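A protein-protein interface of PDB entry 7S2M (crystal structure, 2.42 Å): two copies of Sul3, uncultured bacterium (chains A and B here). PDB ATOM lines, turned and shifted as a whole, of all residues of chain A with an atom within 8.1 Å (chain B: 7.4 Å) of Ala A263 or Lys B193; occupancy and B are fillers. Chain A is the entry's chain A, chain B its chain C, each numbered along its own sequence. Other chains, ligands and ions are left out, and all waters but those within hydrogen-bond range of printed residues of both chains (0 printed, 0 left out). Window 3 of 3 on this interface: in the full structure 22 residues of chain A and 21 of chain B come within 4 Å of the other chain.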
ATOM      1  N   TYR A 239     -13.490   0.079   8.764  1.00  0.00           N
ATOM      2  CA  TYR A 239     -12.810   0.862   7.738  1.00  0.00           C
ATOM      3  C   TYR A 239     -11.302   0.847   7.949  1.00  0.00           C
ATOM      4  O   TYR A 239     -10.535   0.596   7.011  1.00  0.00           O
ATOM      5  CB  TYR A 239     -13.335   2.297   7.733  1.00  0.00           C
ATOM      6  CG  TYR A 239     -12.537   3.223   6.844  1.00  0.00           C
ATOM      7  CD1 TYR A 239     -12.525   3.052   5.467  1.00  0.00           C
ATOM      8  CD2 TYR A 239     -11.790   4.263   7.381  1.00  0.00           C
ATOM      9  CE1 TYR A 239     -11.796   3.892   4.647  1.00  0.00           C
ATOM     10  CE2 TYR A 239     -11.058   5.111   6.571  1.00  0.00           C
ATOM     11  CZ  TYR A 239     -11.064   4.920   5.205  1.00  0.00           C
ATOM     12  OH  TYR A 239     -10.337   5.760   4.393  1.00  0.00           O
ATOM     13  N   ALA A 257     -17.546  11.010   8.276  1.00  0.00           N
ATOM     14  CA  ALA A 257     -16.615  10.398   9.216  1.00  0.00           C
ATOM     15  C   ALA A 257     -15.356   9.913   8.508  1.00  0.00           C
ATOM     16  O   ALA A 257     -14.243  10.079   9.024  1.00  0.00           O
ATOM     17  CB  ALA A 257     -17.297   9.248   9.956  1.00  0.00           C
ATOM     18  N   LEU A 258     -15.510   9.315   7.323  1.00  0.00           N
ATOM     19  CA  LEU A 258     -14.346   8.867   6.563  1.00  0.00           C
ATOM     20  C   LEU A 258     -13.459  10.032   6.155  1.00  0.00           C
ATOM     21  O   LEU A 258     -12.247   9.858   5.980  1.00  0.00           O
ATOM     22  CB  LEU A 258     -14.790   8.092   5.322  1.00  0.00           C
ATOM     23  CG  LEU A 258     -15.441   6.726   5.544  1.00  0.00           C
ATOM     24  CD1 LEU A 258     -15.377   5.887   4.275  1.00  0.00           C
ATOM     25  CD2 LEU A 258     -14.795   6.000   6.712  1.00  0.00           C
ATOM     26  N   LYS A 259     -14.039  11.223   5.990  1.00  0.00           N
ATOM     27  CA  LYS A 259     -13.246  12.389   5.625  1.00  0.00           C
ATOM     28  C   LYS A 259     -12.441  12.927   6.801  1.00  0.00           C
ATOM     29  O   LYS A 259     -11.474  13.666   6.587  1.00  0.00           O
ATOM     30  CB  LYS A 259     -14.154  13.478   5.054  1.00  0.00           C
ATOM     31  CG  LYS A 259     -14.751  13.125   3.698  1.00  0.00           C
ATOM     32  CD  LYS A 259     -15.093  14.364   2.889  1.00  0.00           C
ATOM     33  CE  LYS A 259     -16.505  14.842   3.178  1.00  0.00           C
ATOM     34  NZ  LYS A 259     -16.873  16.027   2.357  1.00  0.00           N
ATOM     35  N   ILE A 260     -12.811  12.570   8.030  1.00  0.00           N
ATOM     36  CA  ILE A 260     -12.030  12.977   9.194  1.00  0.00           C
ATOM     37  C   ILE A 260     -10.845  12.040   9.397  1.00  0.00           C
ATOM     38  O   ILE A 260      -9.718  12.483   9.639  1.00  0.00           O
ATOM     39  CB  ILE A 260     -12.923  13.035  10.447  1.00  0.00           C
ATOM     40  CG1 ILE A 260     -14.030  14.079  10.270  1.00  0.00           C
ATOM     41  CG2 ILE A 260     -12.088  13.331  11.685  1.00  0.00           C
ATOM     42  CD1 ILE A 260     -13.546  15.513  10.340  1.00  0.00           C
ATOM     43  N   SER A 261     -11.085  10.729   9.299  1.00  0.00           N
ATOM     44  CA  SER A 261     -10.008   9.764   9.490  1.00  0.00           C
ATOM     45  C   SER A 261      -8.962   9.856   8.387  1.00  0.00           C
ATOM     46  O   SER A 261      -7.785   9.561   8.626  1.00  0.00           O
ATOM     47  CB  SER A 261     -10.579   8.347   9.561  1.00  0.00           C
ATOM     48  OG  SER A 261     -10.766   7.943  10.907  1.00  0.00           O
ATOM     49  N   LYS A 262      -9.363  10.261   7.181  1.00  0.00           N
ATOM     50  CA  LYS A 262      -8.397  10.415   6.098  1.00  0.00           C
ATOM     51  C   LYS A 262      -7.501  11.626   6.325  1.00  0.00           C
ATOM     52  O   LYS A 262      -6.312  11.602   5.980  1.00  0.00           O
ATOM     53  CB  LYS A 262      -9.124  10.527   4.758  1.00  0.00           C
ATOM     54  CG  LYS A 262      -9.162   9.232   3.959  1.00  0.00           C
ATOM     55  CD  LYS A 262     -10.406   9.136   3.081  1.00  0.00           C
ATOM     56  CE  LYS A 262     -10.923  10.507   2.661  1.00  0.00           C
ATOM     57  NZ  LYS A 262     -12.292  10.431   2.076  1.00  0.00           N
ATOM     58  N   ALA A 263      -8.050  12.694   6.906  1.00  0.00           N
ATOM     59  CA  ALA A 263      -7.248  13.872   7.210  1.00  0.00           C
ATOM     60  C   ALA A 263      -6.398  13.660   8.457  1.00  0.00           C
ATOM     61  O   ALA A 263      -5.253  14.122   8.518  1.00  0.00           O
ATOM     62  CB  ALA A 263      -8.152  15.094   7.379  1.00  0.00           C
ATOM     63  N   LEU A 264      -6.939  12.961   9.455  1.00  0.00           N
ATOM     64  CA  LEU A 264      -6.199  12.696  10.681  1.00  0.00           C
ATOM     65  C   LEU A 264      -5.144  11.612  10.507  1.00  0.00           C
ATOM     66  O   LEU A 264      -4.228  11.520  11.331  1.00  0.00           O
ATOM     67  CB  LEU A 264      -7.170  12.309  11.799  1.00  0.00           C
ATOM     68  CG  LEU A 264      -7.999  13.449  12.397  1.00  0.00           C
ATOM     69  CD1 LEU A 264      -8.593  13.042  13.733  1.00  0.00           C
ATOM     70  CD2 LEU A 264      -7.165  14.713  12.548  1.00  0.00           C
ATOM     71  N   GLY A 265      -5.250  10.798   9.461  1.00  0.00           N
ATOM     72  CA  GLY A 265      -4.281   9.749   9.201  1.00  0.00           C
ATOM     73  C   GLY A 265      -4.404   8.555  10.128  1.00  0.00           C
ATOM     74  O   GLY A 265      -4.035   8.620  11.301  1.00  0.00           O
ATOM     75  OXT GLY A 265      -4.870   7.488   9.727  1.00  0.00           O
ATOM     76  N   PHE B 147       3.464  24.359  17.772  1.00  0.00           N
ATOM     77  CA  PHE B 147       3.663  23.203  18.639  1.00  0.00           C
ATOM     78  C   PHE B 147       4.889  23.380  19.528  1.00  0.00           C
ATOM     79  O   PHE B 147       4.852  23.043  20.717  1.00  0.00           O
ATOM     80  CB  PHE B 147       3.788  21.933  17.796  1.00  0.00           C
ATOM     81  CG  PHE B 147       3.724  20.665  18.598  1.00  0.00           C
ATOM     82  CD1 PHE B 147       4.876  20.096  19.117  1.00  0.00           C
ATOM     83  CD2 PHE B 147       2.508  20.043  18.836  1.00  0.00           C
ATOM     84  CE1 PHE B 147       4.818  18.931  19.857  1.00  0.00           C
ATOM     85  CE2 PHE B 147       2.445  18.877  19.575  1.00  0.00           C
ATOM     86  CZ  PHE B 147       3.601  18.321  20.086  1.00  0.00           C
ATOM     87  N   GLU B 186      -5.129  23.159   9.634  1.00  0.00           N
ATOM     88  CA  GLU B 186      -3.945  22.307   9.690  1.00  0.00           C
ATOM     89  C   GLU B 186      -3.318  22.308  11.077  1.00  0.00           C
ATOM     90  O   GLU B 186      -2.696  21.317  11.478  1.00  0.00           O
ATOM     91  CB  GLU B 186      -2.920  22.766   8.650  1.00  0.00           C
ATOM     92  CG  GLU B 186      -3.028  22.089   7.282  1.00  0.00           C
ATOM     93  CD  GLU B 186      -3.650  20.703   7.332  1.00  0.00           C
ATOM     94  OE1 GLU B 186      -3.131  19.833   8.064  1.00  0.00           O
ATOM     95  OE2 GLU B 186      -4.667  20.486   6.640  1.00  0.00           O
ATOM     96  N   THR B 187      -3.469  23.406  11.820  1.00  0.00           N
ATOM     97  CA  THR B 187      -2.908  23.475  13.163  1.00  0.00           C
ATOM     98  C   THR B 187      -3.594  22.486  14.095  1.00  0.00           C
ATOM     99  O   THR B 187      -2.930  21.796  14.875  1.00  0.00           O
ATOM    100  CB  THR B 187      -3.036  24.894  13.711  1.00  0.00           C
ATOM    101  OG1 THR B 187      -2.844  25.830  12.644  1.00  0.00           O
ATOM    102  CG2 THR B 187      -1.994  25.141  14.789  1.00  0.00           C
ATOM    103  N   SER B 188      -4.925  22.402  14.024  1.00  0.00           N
ATOM    104  CA  SER B 188      -5.653  21.471  14.877  1.00  0.00           C
ATOM    105  C   SER B 188      -5.388  20.025  14.484  1.00  0.00           C
ATOM    106  O   SER B 188      -5.371  19.144  15.352  1.00  0.00           O
ATOM    107  CB  SER B 188      -7.149  21.773  14.827  1.00  0.00           C
ATOM    108  OG  SER B 188      -7.429  23.071  15.324  1.00  0.00           O
ATOM    109  N   ILE B 189      -5.182  19.758  13.193  1.00  0.00           N
ATOM    110  CA  ILE B 189      -4.856  18.403  12.761  1.00  0.00           C
ATOM    111  C   ILE B 189      -3.497  17.984  13.307  1.00  0.00           C
ATOM    112  O   ILE B 189      -3.327  16.855  13.786  1.00  0.00           O
ATOM    113  CB  ILE B 189      -4.905  18.305  11.227  1.00  0.00           C
ATOM    114  CG1 ILE B 189      -6.319  18.580  10.718  1.00  0.00           C
ATOM    115  CG2 ILE B 189      -4.420  16.938  10.761  1.00  0.00           C
ATOM    116  CD1 ILE B 189      -6.386  18.854   9.232  1.00  0.00           C
ATOM    117  N   LEU B 190      -2.513  18.886  13.256  1.00  0.00           N
ATOM    118  CA  LEU B 190      -1.173  18.556  13.735  1.00  0.00           C
ATOM    119  C   LEU B 190      -1.187  18.198  15.215  1.00  0.00           C
ATOM    120  O   LEU B 190      -0.547  17.226  15.632  1.00  0.00           O
ATOM    121  CB  LEU B 190      -0.219  19.724  13.463  1.00  0.00           C
ATOM    122  CG  LEU B 190       1.286  19.596  13.750  1.00  0.00           C
ATOM    123  CD1 LEU B 190       2.050  20.610  12.919  1.00  0.00           C
ATOM    124  CD2 LEU B 190       1.623  19.803  15.225  1.00  0.00           C
ATOM    125  N   VAL B 191      -1.908  18.975  16.026  1.00  0.00           N
ATOM    126  CA  VAL B 191      -1.934  18.715  17.461  1.00  0.00           C
ATOM    127  C   VAL B 191      -2.692  17.431  17.771  1.00  0.00           C
ATOM    128  O   VAL B 191      -2.365  16.728  18.736  1.00  0.00           O
ATOM    129  CB  VAL B 191      -2.535  19.920  18.205  1.00  0.00           C
ATOM    130  CG1 VAL B 191      -2.402  19.732  19.696  1.00  0.00           C
ATOM    131  CG2 VAL B 191      -1.838  21.198  17.775  1.00  0.00           C
ATOM    132  N   LEU B 192      -3.706  17.096  16.971  1.00  0.00           N
ATOM    133  CA  LEU B 192      -4.437  15.856  17.203  1.00  0.00           C
ATOM    134  C   LEU B 192      -3.577  14.634  16.906  1.00  0.00           C
ATOM    135  O   LEU B 192      -3.812  13.560  17.471  1.00  0.00           O
ATOM    136  CB  LEU B 192      -5.714  15.830  16.363  1.00  0.00           C
ATOM    137  CG  LEU B 192      -6.962  16.393  17.045  1.00  0.00           C
ATOM    138  CD1 LEU B 192      -8.088  16.573  16.041  1.00  0.00           C
ATOM    139  CD2 LEU B 192      -7.396  15.491  18.190  1.00  0.00           C
ATOM    140  N   LYS B 193      -2.578  14.774  16.034  1.00  0.00           N
ATOM    141  CA  LYS B 193      -1.684  13.671  15.712  1.00  0.00           C
ATOM    142  C   LYS B 193      -0.478  13.584  16.634  1.00  0.00           C
ATOM    143  O   LYS B 193       0.179  12.538  16.673  1.00  0.00           O
ATOM    144  CB  LYS B 193      -1.181  13.789  14.268  1.00  0.00           C
ATOM    145  CG  LYS B 193      -2.268  13.905  13.212  1.00  0.00           C
ATOM    146  CD  LYS B 193      -1.703  14.487  11.924  1.00  0.00           C
ATOM    147  CE  LYS B 193      -1.598  13.436  10.827  1.00  0.00           C
ATOM    148  NZ  LYS B 193      -1.784  14.025   9.470  1.00  0.00           N
ATOM    149  N   ARG B 194      -0.169  14.648  17.375  1.00  0.00           N
ATOM    150  CA  ARG B 194       1.086  14.737  18.111  1.00  0.00           C
ATOM    151  C   ARG B 194       0.888  15.000  19.598  1.00  0.00           C
ATOM    152  O   ARG B 194       1.865  15.300  20.297  1.00  0.00           O
ATOM    153  CB  ARG B 194       1.969  15.828  17.494  1.00  0.00           C
ATOM    154  CG  ARG B 194       2.645  15.402  16.197  1.00  0.00           C
ATOM    155  CD  ARG B 194       3.818  16.299  15.824  1.00  0.00           C
ATOM    156  NE  ARG B 194       4.888  16.288  16.813  1.00  0.00           N
ATOM    157  CZ  ARG B 194       5.773  17.265  16.965  1.00  0.00           C
ATOM    158  NH1 ARG B 194       5.752  18.340  16.194  1.00  0.00           N
ATOM    159  NH2 ARG B 194       6.705  17.158  17.907  1.00  0.00           N
ATOM    160  N   PHE B 195      -0.337  14.892  20.107  1.00  0.00           N
ATOM    161  CA  PHE B 195      -0.554  15.128  21.528  1.00  0.00           C
ATOM    162  C   PHE B 195      -0.005  14.007  22.415  1.00  0.00           C
ATOM    163  O   PHE B 195       0.224  14.256  23.607  1.00  0.00           O
ATOM    164  CB  PHE B 195      -2.042  15.383  21.817  1.00  0.00           C
ATOM    165  CG  PHE B 195      -2.903  14.146  21.828  1.00  0.00           C
ATOM    166  CD1 PHE B 195      -3.495  13.686  20.662  1.00  0.00           C
ATOM    167  CD2 PHE B 195      -3.140  13.460  23.010  1.00  0.00           C
ATOM    168  CE1 PHE B 195      -4.289  12.557  20.671  1.00  0.00           C
ATOM    169  CE2 PHE B 195      -3.933  12.331  23.024  1.00  0.00           C
ATOM    170  CZ  PHE B 195      -4.509  11.879  21.855  1.00  0.00           C
ATOM    171  N   PRO B 196       0.219  12.779  21.921  1.00  0.00           N
ATOM    172  CA  PRO B 196       0.988  11.828  22.742  1.00  0.00           C
ATOM    173  C   PRO B 196       2.373  12.328  23.114  1.00  0.00           C
ATOM    174  O   PRO B 196       2.916  11.912  24.146  1.00  0.00           O
ATOM    175  CB  PRO B 196       1.068  10.573  21.863  1.00  0.00           C
ATOM    176  CG  PRO B 196      -0.048  10.662  20.929  1.00  0.00           C
ATOM    177  CD  PRO B 196      -0.530  12.079  20.858  1.00  0.00           C
ATOM    178  N   GLU B 197       2.967  13.209  22.305  1.00  0.00           N
ATOM    179  CA  GLU B 197       4.286  13.736  22.640  1.00  0.00           C
ATOM    180  C   GLU B 197       4.232  14.602  23.892  1.00  0.00           C
ATOM    181  O   GLU B 197       5.176  14.606  24.692  1.00  0.00           O
ATOM    182  CB  GLU B 197       4.852  14.523  21.461  1.00  0.00           C
ATOM    183  CG  GLU B 197       5.459  13.647  20.379  1.00  0.00           C
ATOM    184  CD  GLU B 197       5.933  14.448  19.185  1.00  0.00           C
ATOM    185  OE1 GLU B 197       6.809  15.319  19.370  1.00  0.00           O
ATOM    186  OE2 GLU B 197       5.436  14.208  18.065  1.00  0.00           O
ATOM    187  N   ILE B 219     -12.995  20.470   6.935  1.00  0.00           N
ATOM    188  CA  ILE B 219     -12.445  19.229   6.412  1.00  0.00           C
ATOM    189  C   ILE B 219     -13.498  18.418   5.669  1.00  0.00           C
ATOM    190  O   ILE B 219     -13.204  17.807   4.641  1.00  0.00           O
ATOM    191  CB  ILE B 219     -11.821  18.409   7.562  1.00  0.00           C
ATOM    192  CG1 ILE B 219     -10.709  19.207   8.250  1.00  0.00           C
ATOM    193  CG2 ILE B 219     -11.296  17.075   7.053  1.00  0.00           C
ATOM    194  CD1 ILE B 219     -10.147  18.525   9.483  1.00  0.00           C
ATOM    195  N   TYR B 237     -10.650   8.849  17.540  1.00  0.00           N
ATOM    196  CA  TYR B 237      -9.235   8.951  17.203  1.00  0.00           C
ATOM    197  C   TYR B 237      -8.411   9.389  18.407  1.00  0.00           C
ATOM    198  O   TYR B 237      -7.319   8.861  18.647  1.00  0.00           O
ATOM    199  CB  TYR B 237      -9.057   9.928  16.038  1.00  0.00           C
ATOM    200  CG  TYR B 237      -7.624  10.214  15.639  1.00  0.00           C
ATOM    201  CD1 TYR B 237      -6.913  11.259  16.219  1.00  0.00           C
ATOM    202  CD2 TYR B 237      -6.991   9.453  14.666  1.00  0.00           C
ATOM    203  CE1 TYR B 237      -5.609  11.527  15.847  1.00  0.00           C
ATOM    204  CE2 TYR B 237      -5.688   9.714  14.289  1.00  0.00           C
ATOM    205  CZ  TYR B 237      -5.002  10.752  14.882  1.00  0.00           C
ATOM    206  OH  TYR B 237      -3.703  11.013  14.508  1.00  0.00           O
ATOM    207  N   LYS B 241      -5.561   6.996  20.727  1.00  0.00           N
ATOM    208  CA  LYS B 241      -4.177   7.426  20.872  1.00  0.00           C
ATOM    209  C   LYS B 241      -3.795   7.727  22.317  1.00  0.00           C
ATOM    210  O   LYS B 241      -2.673   8.179  22.564  1.00  0.00           O
ATOM    211  CB  LYS B 241      -3.908   8.655  19.999  1.00  0.00           C
ATOM    212  CG  LYS B 241      -4.123   8.410  18.515  1.00  0.00           C
ATOM    213  CD  LYS B 241      -3.323   9.385  17.668  1.00  0.00           C
ATOM    214  CE  LYS B 241      -1.902   8.895  17.458  1.00  0.00           C
ATOM    215  NZ  LYS B 241      -1.205   9.666  16.392  1.00  0.00           N
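O of Leu A264 is in hydrogen-bond range of OH of Tyr B237 (3.3 Å).
The backbone carbonyl oxygen (O) of Lys B193 lies within hydrogen-bond range of the side-chain amino group (NZ) of Lys B241, 3.2 Å away.
OH of Tyr B237 lies within hydrogen-bond range of NZ of Lys B241 (3.4 Å).
Among the printed residues, pairs that only touch across the chains: Lys A259 with Ile B219, Ala A263 with Ile B189, Ala A263 with Lys B193, Ala A263 with Ile B219, Leu A264 with Ile B189, Leu A264 with Lys B193 and Gly A265 with Tyr B237.
Of chain B, only Ile B189 (3.7 Å), Lys B193 (3.6 Å) and Ile B219 (3.7 Å) come within 4 Å of Ala A263.
Of chain A, only Ala A263 (3.6 Å) and Leu A264 (3.3 Å) come within 4 Å of Lys B193.
Of the printed residues of chain B, Gly A265 touches Tyr B237 (3.6 Å).
Printed residues of chain A within 4 Å of Ile B219: Lys A259 and Ala A263.
Leu B190 touches none of the printed residues of chain A.
Tyr A239 touches none of the printed residues of chain B.
Of the 16 printed residues of chain B, 4 touch a printed residue of chain A.
Hydrophobic or aromatic side chains of chain B that line the printed part of chain A: Ile B189, Ile B219 and Tyr B237.
Of the 10 printed residues of chain A, 4 touch a printed residue of chain B.
Hydrophobic or aromatic side chains of chain A that line the printed part of chain B: Ala A263 and Leu A264.
Among the printed residues, 8 pairs touch across the chains.
No position is printed for both chains.
Of the 8 pairs that touch across the chains among the printed residues, none has its exchanged pair printed and touching as well.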
